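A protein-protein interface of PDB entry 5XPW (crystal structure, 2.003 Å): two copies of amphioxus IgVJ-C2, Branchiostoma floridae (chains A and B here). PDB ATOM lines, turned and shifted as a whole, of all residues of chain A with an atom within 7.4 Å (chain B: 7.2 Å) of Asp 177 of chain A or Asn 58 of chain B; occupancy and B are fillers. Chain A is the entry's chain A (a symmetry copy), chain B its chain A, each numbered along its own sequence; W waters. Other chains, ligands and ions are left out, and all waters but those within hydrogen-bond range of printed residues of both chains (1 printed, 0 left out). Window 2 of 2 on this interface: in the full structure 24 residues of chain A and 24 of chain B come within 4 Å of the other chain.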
ATOM      1  N   PRO A 110     -12.453   6.967 -18.713  1.00  0.00           N
ATOM      2  CA  PRO A 110     -13.403   6.380 -17.765  1.00  0.00           C
ATOM      3  C   PRO A 110     -14.581   7.322 -17.560  1.00  0.00           C
ATOM      4  O   PRO A 110     -14.446   8.520 -17.806  1.00  0.00           O
ATOM      5  CB  PRO A 110     -12.595   6.283 -16.462  1.00  0.00           C
ATOM      6  CG  PRO A 110     -11.171   6.564 -16.832  1.00  0.00           C
ATOM      7  CD  PRO A 110     -11.227   7.432 -18.045  1.00  0.00           C
ATOM      8  N   TYR A 111     -15.718   6.794 -17.119  1.00  0.00           N
ATOM      9  CA  TYR A 111     -16.872   7.638 -16.819  1.00  0.00           C
ATOM     10  C   TYR A 111     -16.966   7.929 -15.322  1.00  0.00           C
ATOM     11  O   TYR A 111     -17.763   8.758 -14.888  1.00  0.00           O
ATOM     12  CB  TYR A 111     -18.160   7.018 -17.364  1.00  0.00           C
ATOM     13  CG  TYR A 111     -18.137   6.881 -18.873  1.00  0.00           C
ATOM     14  CD1 TYR A 111     -17.950   5.648 -19.476  1.00  0.00           C
ATOM     15  CD2 TYR A 111     -18.275   7.996 -19.692  1.00  0.00           C
ATOM     16  CE1 TYR A 111     -17.918   5.519 -20.856  1.00  0.00           C
ATOM     17  CE2 TYR A 111     -18.245   7.882 -21.072  1.00  0.00           C
ATOM     18  CZ  TYR A 111     -18.066   6.640 -21.649  1.00  0.00           C
ATOM     19  OH  TYR A 111     -18.035   6.515 -23.018  1.00  0.00           O
ATOM     20  N   GLU A 112     -16.141   7.234 -14.544  1.00  0.00           N
ATOM     21  CA  GLU A 112     -15.884   7.608 -13.161  1.00  0.00           C
ATOM     22  C   GLU A 112     -14.455   8.122 -13.107  1.00  0.00           C
ATOM     23  O   GLU A 112     -13.511   7.361 -13.316  1.00  0.00           O
ATOM     24  CB  GLU A 112     -16.034   6.408 -12.230  1.00  0.00           C
ATOM     25  CG  GLU A 112     -17.362   5.686 -12.344  1.00  0.00           C
ATOM     26  CD  GLU A 112     -17.410   4.444 -11.478  1.00  0.00           C
ATOM     27  OE1 GLU A 112     -17.223   3.337 -12.024  1.00  0.00           O
ATOM     28  OE2 GLU A 112     -17.618   4.577 -10.254  1.00  0.00           O
ATOM     29  N   MET A 119     -10.555  12.055 -19.070  1.00  0.00           N
ATOM     30  CA  MET A 119     -11.334  11.051 -19.784  1.00  0.00           C
ATOM     31  C   MET A 119     -11.519  11.487 -21.231  1.00  0.00           C
ATOM     32  O   MET A 119     -11.366  12.665 -21.554  1.00  0.00           O
ATOM     33  CB  MET A 119     -12.697  10.824 -19.116  1.00  0.00           C
ATOM     34  CG  MET A 119     -13.690  11.990 -19.238  1.00  0.00           C
ATOM     35  SD  MET A 119     -14.604  12.045 -20.801  1.00  0.00           S
ATOM     36  CE  MET A 119     -15.323  10.408 -20.816  1.00  0.00           C
ATOM     37  N   GLU A 157     -17.552  19.404 -13.622  1.00  0.00           N
ATOM     38  CA  GLU A 157     -17.635  18.617 -14.848  1.00  0.00           C
ATOM     39  C   GLU A 157     -18.598  17.438 -14.722  1.00  0.00           C
ATOM     40  O   GLU A 157     -18.987  16.844 -15.726  1.00  0.00           O
ATOM     41  CB  GLU A 157     -16.253  18.096 -15.246  1.00  0.00           C
ATOM     42  CG  GLU A 157     -15.101  18.995 -14.830  1.00  0.00           C
ATOM     43  CD  GLU A 157     -14.820  20.086 -15.834  1.00  0.00           C
ATOM     44  OE1 GLU A 157     -15.044  21.271 -15.503  1.00  0.00           O
ATOM     45  OE2 GLU A 157     -14.370  19.758 -16.951  1.00  0.00           O
ATOM     46  N   ILE A 158     -18.966  17.086 -13.495  1.00  0.00           N
ATOM     47  CA  ILE A 158     -19.865  15.957 -13.299  1.00  0.00           C
ATOM     48  C   ILE A 158     -21.266  16.288 -13.815  1.00  0.00           C
ATOM     49  O   ILE A 158     -21.767  17.398 -13.627  1.00  0.00           O
ATOM     50  CB  ILE A 158     -19.909  15.474 -11.820  1.00  0.00           C
ATOM     51  CG1 ILE A 158     -21.326  15.556 -11.254  1.00  0.00           C
ATOM     52  CG2 ILE A 158     -18.922  16.249 -10.955  1.00  0.00           C
ATOM     53  CD1 ILE A 158     -22.110  14.266 -11.397  1.00  0.00           C
ATOM     54  N   GLY A 159     -21.883  15.321 -14.486  1.00  0.00           N
ATOM     55  CA  GLY A 159     -23.226  15.494 -15.004  1.00  0.00           C
ATOM     56  C   GLY A 159     -23.486  14.632 -16.224  1.00  0.00           C
ATOM     57  O   GLY A 159     -22.685  13.761 -16.569  1.00  0.00           O
ATOM     58  N   THR A 160     -24.613  14.882 -16.881  1.00  0.00           N
ATOM     59  CA  THR A 160     -24.991  14.119 -18.061  1.00  0.00           C
ATOM     60  C   THR A 160     -24.478  14.756 -19.351  1.00  0.00           C
ATOM     61  O   THR A 160     -24.703  15.941 -19.605  1.00  0.00           O
ATOM     62  CB  THR A 160     -26.516  13.961 -18.148  1.00  0.00           C
ATOM     63  OG1 THR A 160     -26.990  13.307 -16.966  1.00  0.00           O
ATOM     64  CG2 THR A 160     -26.898  13.137 -19.366  1.00  0.00           C
ATOM     65  N   TYR A 161     -23.785  13.958 -20.157  1.00  0.00           N
ATOM     66  CA  TYR A 161     -23.266  14.393 -21.450  1.00  0.00           C
ATOM     67  C   TYR A 161     -23.997  13.659 -22.567  1.00  0.00           C
ATOM     68  O   TYR A 161     -24.263  12.462 -22.455  1.00  0.00           O
ATOM     69  CB  TYR A 161     -21.771  14.101 -21.543  1.00  0.00           C
ATOM     70  CG  TYR A 161     -20.919  14.951 -20.626  1.00  0.00           C
ATOM     71  CD1 TYR A 161     -20.099  15.948 -21.140  1.00  0.00           C
ATOM     72  CD2 TYR A 161     -20.934  14.757 -19.251  1.00  0.00           C
ATOM     73  CE1 TYR A 161     -19.317  16.729 -20.312  1.00  0.00           C
ATOM     74  CE2 TYR A 161     -20.153  15.533 -18.410  1.00  0.00           C
ATOM     75  CZ  TYR A 161     -19.346  16.518 -18.949  1.00  0.00           C
ATOM     76  OH  TYR A 161     -18.567  17.297 -18.129  1.00  0.00           O
ATOM     77  N   SER A 175     -26.923   9.529 -24.110  1.00  0.00           N
ATOM     78  CA  SER A 175     -26.480  10.269 -22.938  1.00  0.00           C
ATOM     79  C   SER A 175     -25.738   9.347 -21.988  1.00  0.00           C
ATOM     80  O   SER A 175     -26.153   8.210 -21.764  1.00  0.00           O
ATOM     81  CB  SER A 175     -27.679  10.885 -22.208  1.00  0.00           C
ATOM     82  OG  SER A 175     -28.388  11.786 -23.040  1.00  0.00           O
ATOM     83  N   VAL A 176     -24.641   9.841 -21.431  1.00  0.00           N
ATOM     84  CA  VAL A 176     -23.906   9.105 -20.412  1.00  0.00           C
ATOM     85  C   VAL A 176     -23.510  10.038 -19.277  1.00  0.00           C
ATOM     86  O   VAL A 176     -23.257  11.223 -19.495  1.00  0.00           O
ATOM     87  CB  VAL A 176     -22.646   8.413 -20.982  1.00  0.00           C
ATOM     88  CG1 VAL A 176     -23.039   7.288 -21.931  1.00  0.00           C
ATOM     89  CG2 VAL A 176     -21.736   9.422 -21.676  1.00  0.00           C
ATOM     90  N   ASP A 177     -23.469   9.499 -18.065  1.00  0.00           N
ATOM     91  CA  ASP A 177     -23.057  10.268 -16.898  1.00  0.00           C
ATOM     92  C   ASP A 177     -21.553  10.214 -16.708  1.00  0.00           C
ATOM     93  O   ASP A 177     -20.943   9.149 -16.800  1.00  0.00           O
ATOM     94  CB  ASP A 177     -23.730   9.734 -15.638  1.00  0.00           C
ATOM     95  CG  ASP A 177     -25.173  10.169 -15.516  1.00  0.00           C
ATOM     96  OD1 ASP A 177     -25.504  11.283 -15.972  1.00  0.00           O
ATOM     97  OD2 ASP A 177     -25.972   9.394 -14.952  1.00  0.00           O
ATOM     98  N   ILE A 178     -20.959  11.372 -16.448  1.00  0.00           N
ATOM     99  CA  ILE A 178     -19.581  11.424 -15.994  1.00  0.00           C
ATOM    100  C   ILE A 178     -19.576  11.896 -14.544  1.00  0.00           C
ATOM    101  O   ILE A 178     -20.041  12.996 -14.240  1.00  0.00           O
ATOM    102  CB  ILE A 178     -18.726  12.349 -16.867  1.00  0.00           C
ATOM    103  CG1 ILE A 178     -18.694  11.827 -18.306  1.00  0.00           C
ATOM    104  CG2 ILE A 178     -17.312  12.455 -16.312  1.00  0.00           C
ATOM    105  CD1 ILE A 178     -17.857  12.656 -19.233  1.00  0.00           C
ATOM    106  N   THR A 179     -19.077  11.045 -13.653  1.00  0.00           N
ATOM    107  CA  THR A 179     -19.049  11.347 -12.226  1.00  0.00           C
ATOM    108  C   THR A 179     -17.631  11.235 -11.677  1.00  0.00           C
ATOM    109  O   THR A 179     -16.720  10.782 -12.372  1.00  0.00           O
ATOM    110  CB  THR A 179     -19.952  10.380 -11.438  1.00  0.00           C
ATOM    111  OG1 THR A 179     -19.456   9.043 -11.581  1.00  0.00           O
ATOM    112  CG2 THR A 179     -21.386  10.442 -11.953  1.00  0.00           C
ATOM    113  N   LEU B  10     -34.333   8.379 -24.202  1.00  0.00           N
ATOM    114  CA  LEU B  10     -34.238   8.695 -22.787  1.00  0.00           C
ATOM    115  C   LEU B  10     -35.561   9.256 -22.257  1.00  0.00           C
ATOM    116  O   LEU B  10     -36.041  10.289 -22.726  1.00  0.00           O
ATOM    117  CB  LEU B  10     -33.087   9.676 -22.540  1.00  0.00           C
ATOM    118  CG  LEU B  10     -32.825  10.097 -21.089  1.00  0.00           C
ATOM    119  CD1 LEU B  10     -31.391  10.572 -20.913  1.00  0.00           C
ATOM    120  CD2 LEU B  10     -33.807  11.174 -20.642  1.00  0.00           C
ATOM    121  N   TYR B  22     -34.572   8.777  -1.322  1.00  0.00           N
ATOM    122  CA  TYR B  22     -35.751   8.511  -2.133  1.00  0.00           C
ATOM    123  C   TYR B  22     -35.605   7.235  -2.937  1.00  0.00           C
ATOM    124  O   TYR B  22     -34.505   6.709  -3.110  1.00  0.00           O
ATOM    125  CB  TYR B  22     -36.035   9.687  -3.070  1.00  0.00           C
ATOM    126  CG  TYR B  22     -34.851  10.060  -3.930  1.00  0.00           C
ATOM    127  CD1 TYR B  22     -33.930  11.003  -3.500  1.00  0.00           C
ATOM    128  CD2 TYR B  22     -34.648   9.461  -5.166  1.00  0.00           C
ATOM    129  CE1 TYR B  22     -32.839  11.345  -4.280  1.00  0.00           C
ATOM    130  CE2 TYR B  22     -33.559   9.795  -5.950  1.00  0.00           C
ATOM    131  CZ  TYR B  22     -32.659  10.740  -5.499  1.00  0.00           C
ATOM    132  OH  TYR B  22     -31.573  11.082  -6.271  1.00  0.00           O
ATOM    133  N   ILE B  24     -36.812   5.479  -6.701  1.00  0.00           N
ATOM    134  CA  ILE B  24     -37.390   5.699  -8.017  1.00  0.00           C
ATOM    135  C   ILE B  24     -37.689   4.358  -8.669  1.00  0.00           C
ATOM    136  O   ILE B  24     -36.878   3.436  -8.611  1.00  0.00           O
ATOM    137  CB  ILE B  24     -36.452   6.527  -8.920  1.00  0.00           C
ATOM    138  CG1 ILE B  24     -36.283   7.940  -8.357  1.00  0.00           C
ATOM    139  CG2 ILE B  24     -36.990   6.596 -10.341  1.00  0.00           C
ATOM    140  CD1 ILE B  24     -35.363   8.814  -9.168  1.00  0.00           C
ATOM    141  N   TYR B  36     -34.647   1.838  -7.873  1.00  0.00           N
ATOM    142  CA  TYR B  36     -33.435   2.502  -7.414  1.00  0.00           C
ATOM    143  C   TYR B  36     -33.636   3.186  -6.068  1.00  0.00           C
ATOM    144  O   TYR B  36     -34.560   3.979  -5.897  1.00  0.00           O
ATOM    145  CB  TYR B  36     -32.960   3.521  -8.448  1.00  0.00           C
ATOM    146  CG  TYR B  36     -31.898   4.479  -7.952  1.00  0.00           C
ATOM    147  CD1 TYR B  36     -30.563   4.095  -7.881  1.00  0.00           C
ATOM    148  CD2 TYR B  36     -32.227   5.774  -7.575  1.00  0.00           C
ATOM    149  CE1 TYR B  36     -29.591   4.971  -7.434  1.00  0.00           C
ATOM    150  CE2 TYR B  36     -31.262   6.655  -7.130  1.00  0.00           C
ATOM    151  CZ  TYR B  36     -29.947   6.248  -7.062  1.00  0.00           C
ATOM    152  OH  TYR B  36     -28.987   7.130  -6.622  1.00  0.00           O
ATOM    153  N   GLN B  55     -29.515   2.264 -19.346  1.00  0.00           N
ATOM    154  CA  GLN B  55     -28.785   3.156 -18.459  1.00  0.00           C
ATOM    155  C   GLN B  55     -29.720   3.952 -17.565  1.00  0.00           C
ATOM    156  O   GLN B  55     -30.826   4.313 -17.966  1.00  0.00           O
ATOM    157  CB  GLN B  55     -27.922   4.131 -19.256  1.00  0.00           C
ATOM    158  CG  GLN B  55     -26.768   3.503 -20.006  1.00  0.00           C
ATOM    159  CD  GLN B  55     -25.836   4.547 -20.583  1.00  0.00           C
ATOM    160  OE1 GLN B  55     -24.966   5.067 -19.885  1.00  0.00           O
ATOM    161  NE2 GLN B  55     -26.019   4.867 -21.860  1.00  0.00           N
ATOM    162  N   PHE B  56     -29.250   4.231 -16.354  1.00  0.00           N
ATOM    163  CA  PHE B  56     -29.947   5.097 -15.422  1.00  0.00           C
ATOM    164  C   PHE B  56     -29.104   6.352 -15.300  1.00  0.00           C
ATOM    165  O   PHE B  56     -28.020   6.328 -14.717  1.00  0.00           O
ATOM    166  CB  PHE B  56     -30.094   4.396 -14.067  1.00  0.00           C
ATOM    167  CG  PHE B  56     -30.874   5.180 -13.044  1.00  0.00           C
ATOM    168  CD1 PHE B  56     -32.157   5.626 -13.315  1.00  0.00           C
ATOM    169  CD2 PHE B  56     -30.335   5.432 -11.791  1.00  0.00           C
ATOM    170  CE1 PHE B  56     -32.875   6.334 -12.366  1.00  0.00           C
ATOM    171  CE2 PHE B  56     -31.044   6.137 -10.839  1.00  0.00           C
ATOM    172  CZ  PHE B  56     -32.319   6.588 -11.126  1.00  0.00           C
ATOM    173  N   VAL B  57     -29.591   7.452 -15.866  1.00  0.00           N
ATOM    174  CA  VAL B  57     -28.773   8.650 -15.968  1.00  0.00           C
ATOM    175  C   VAL B  57     -29.255   9.756 -15.036  1.00  0.00           C
ATOM    176  O   VAL B  57     -30.457   9.932 -14.831  1.00  0.00           O
ATOM    177  CB  VAL B  57     -28.698   9.153 -17.432  1.00  0.00           C
ATOM    178  CG1 VAL B  57     -28.686   7.970 -18.382  1.00  0.00           C
ATOM    179  CG2 VAL B  57     -29.862  10.068 -17.754  1.00  0.00           C
ATOM    180  N   ASN B  58     -28.303  10.480 -14.456  1.00  0.00           N
ATOM    181  CA  ASN B  58     -28.597  11.584 -13.544  1.00  0.00           C
ATOM    182  C   ASN B  58     -29.458  11.185 -12.338  1.00  0.00           C
ATOM    183  O   ASN B  58     -30.197  12.008 -11.797  1.00  0.00           O
ATOM    184  CB  ASN B  58     -29.249  12.745 -14.305  1.00  0.00           C
ATOM    185  CG  ASN B  58     -29.324  14.015 -13.482  1.00  0.00           C
ATOM    186  OD1 ASN B  58     -28.378  14.372 -12.779  1.00  0.00           O
ATOM    187  ND2 ASN B  58     -30.454  14.710 -13.569  1.00  0.00           N
ATOM    188  N   ASN B  59     -29.350   9.926 -11.919  1.00  0.00           N
ATOM    189  CA  ASN B  59     -30.122   9.425 -10.780  1.00  0.00           C
ATOM    190  C   ASN B  59     -31.626   9.640 -10.944  1.00  0.00           C
ATOM    191  O   ASN B  59     -32.356   9.705  -9.955  1.00  0.00           O
ATOM    192  CB  ASN B  59     -29.660  10.092  -9.479  1.00  0.00           C
ATOM    193  CG  ASN B  59     -28.174   9.922  -9.224  1.00  0.00           C
ATOM    194  OD1 ASN B  59     -27.628   8.826  -9.361  1.00  0.00           O
ATOM    195  ND2 ASN B  59     -27.512  11.011  -8.845  1.00  0.00           N
ATOM    196  N   ARG B  60     -32.086   9.754 -12.188  1.00  0.00           N
ATOM    197  CA  ARG B  60     -33.482  10.089 -12.469  1.00  0.00           C
ATOM    198  C   ARG B  60     -34.042   9.315 -13.659  1.00  0.00           C
ATOM    199  O   ARG B  60     -35.061   8.632 -13.553  1.00  0.00           O
ATOM    200  CB  ARG B  60     -33.613  11.584 -12.781  1.00  0.00           C
ATOM    201  CG  ARG B  60     -33.234  12.527 -11.653  1.00  0.00           C
ATOM    202  CD  ARG B  60     -34.319  12.598 -10.599  1.00  0.00           C
ATOM    203  NE  ARG B  60     -34.026  13.605  -9.583  1.00  0.00           N
ATOM    204  CZ  ARG B  60     -33.198  13.412  -8.561  1.00  0.00           C
ATOM    205  NH1 ARG B  60     -32.571  12.251  -8.426  1.00  0.00           N
ATOM    206  NH2 ARG B  60     -32.992  14.381  -7.677  1.00  0.00           N
ATOM    207  N   ASN B  61     -33.353   9.432 -14.792  1.00  0.00           N
ATOM    208  CA  ASN B  61     -33.923   9.095 -16.092  1.00  0.00           C
ATOM    209  C   ASN B  61     -33.549   7.723 -16.636  1.00  0.00           C
ATOM    210  O   ASN B  61     -32.422   7.259 -16.464  1.00  0.00           O
ATOM    211  CB  ASN B  61     -33.533  10.174 -17.100  1.00  0.00           C
ATOM    212  CG  ASN B  61     -33.828  11.570 -16.593  1.00  0.00           C
ATOM    213  OD1 ASN B  61     -34.838  11.794 -15.932  1.00  0.00           O
ATOM    214  ND2 ASN B  61     -32.942  12.514 -16.894  1.00  0.00           N
ATOM    215  N   GLU B  63     -32.806   5.223 -19.773  1.00  0.00           N
ATOM    216  CA  GLU B  63     -32.368   5.223 -21.166  1.00  0.00           C
ATOM    217  C   GLU B  63     -32.209   3.814 -21.739  1.00  0.00           C
ATOM    218  O   GLU B  63     -31.624   2.932 -21.109  1.00  0.00           O
ATOM    219  CB  GLU B  63     -31.061   6.008 -21.329  1.00  0.00           C
ATOM    220  CG  GLU B  63     -30.655   6.221 -22.780  1.00  0.00           C
ATOM    221  CD  GLU B  63     -29.376   7.028 -22.910  1.00  0.00           C
ATOM    222  OE1 GLU B  63     -28.474   6.870 -22.058  1.00  0.00           O
ATOM    223  OE2 GLU B  63     -29.273   7.818 -23.866  1.00  0.00           O
HETATM  224  O   HOH W   1     -27.412   7.791 -12.361  1.00  0.00           O
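Water W1 lies within hydrogen-bond range of O of Phe 56 of chain B (2.8 Å), N of Asn 59 of chain B (2.9 Å) and OD2 of Asp 177 of chain A (3.4 Å).
No position is printed for both chains.
Of the 8 pairs that touch across the chains among the printed residues, none has its exchanged pair printed and touching as well.
The backbone carbonyl oxygen (O) of Glu 63 of chain B sits at hydrogen-bond distance from the backbone NH (N) of Gln 55 of chain B (2.8 Å).
The side-chain hydroxyl (OG1) of Thr 160 of chain A sits at hydrogen-bond distance from the side-chain carboxylate (OD1) of Asp 177 of chain A, at 2.7 Å.
N of Val 176 of chain A is in hydrogen-bond range of O of Tyr 161 of chain A (2.8 Å).
Printed residues of chain A that touch a printed residue of chain B: Thr 160, Ser 175, Val 176 and Asp 177.
Hydrophobic or aromatic side chains of chain A that line the printed part of chain B: Val 176.
Of the 12 printed residues of chain B, 6 touch a printed residue of chain A.
Printed residues of chain B that touch a printed residue of chain A: Leu 10, Gln 55, Phe 56, Val 57, Asn 58 and Glu 63.
Hydrophobic or aromatic side chains of chain B within 4 Å of the printed part of chain A: Leu 10 and Val 57.
Among the printed residues, 8 pairs touch across the chains.
The backbone carbonyl oxygen (O) of Ser 175 of chain A lies within hydrogen-bond range of the side-chain amide nitrogen (NE2) of Gln 55 of chain B.
N of Asn 58 of chain B sits at hydrogen-bond distance from OD2 of Asp 177 of chain A, at 2.6 Å.
The backbone NH (N) of Ser 175 of chain A lies within hydrogen-bond range of the side-chain carboxylate (OE2) of Glu 63 of chain B.
Of chain B, only Phe 56 (3.7 Å), Val 57 (3.1 Å) and Asn 58 (2.6 Å) come within 4 Å of Asp 177 of chain A.
Asn 58 of chain B touches two residues of chain A.
Of the printed residues of chain A, Phe 56 of chain B touches Asp 177.
Of the printed residues of chain A, Val 57 of chain B touches Asp 177.
Printed residues of chain A within 4 Å of Glu 63 of chain B: Ser 175.
Printed residues of chain B within 4 Å of Ser 175 of chain A: Leu 10 (3.9 Å), Gln 55 (3.3 Å) and Glu 63 (2.7 Å).
Of the printed residues of chain A, Gln 55 of chain B touches Ser 175 and Val 176.
Tyr 111 of chain A touches none of the printed residues of chain B.
The nearest residue of chain B that does not touch Asp 177 of chain A is Asn 59 of chain B (4.6 Å).
The nearest residue of chain A that does not touch Asn 58 of chain B is Gly 159 of chain A (5.7 Å).
Asn 58 of chain B touches Thr 160 of chain A.
OG of Ser 175 of chain A touches CD1 of Leu 10 of chain B (3.9 Å).
Val 176 of chain A touches Gln 55 of chain B.
Asp 177 of chain A touches Phe 56 of chain B (OD2 to O, 3.7 Å).
Asp 177 of chain A touches Val 57 of chain B.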
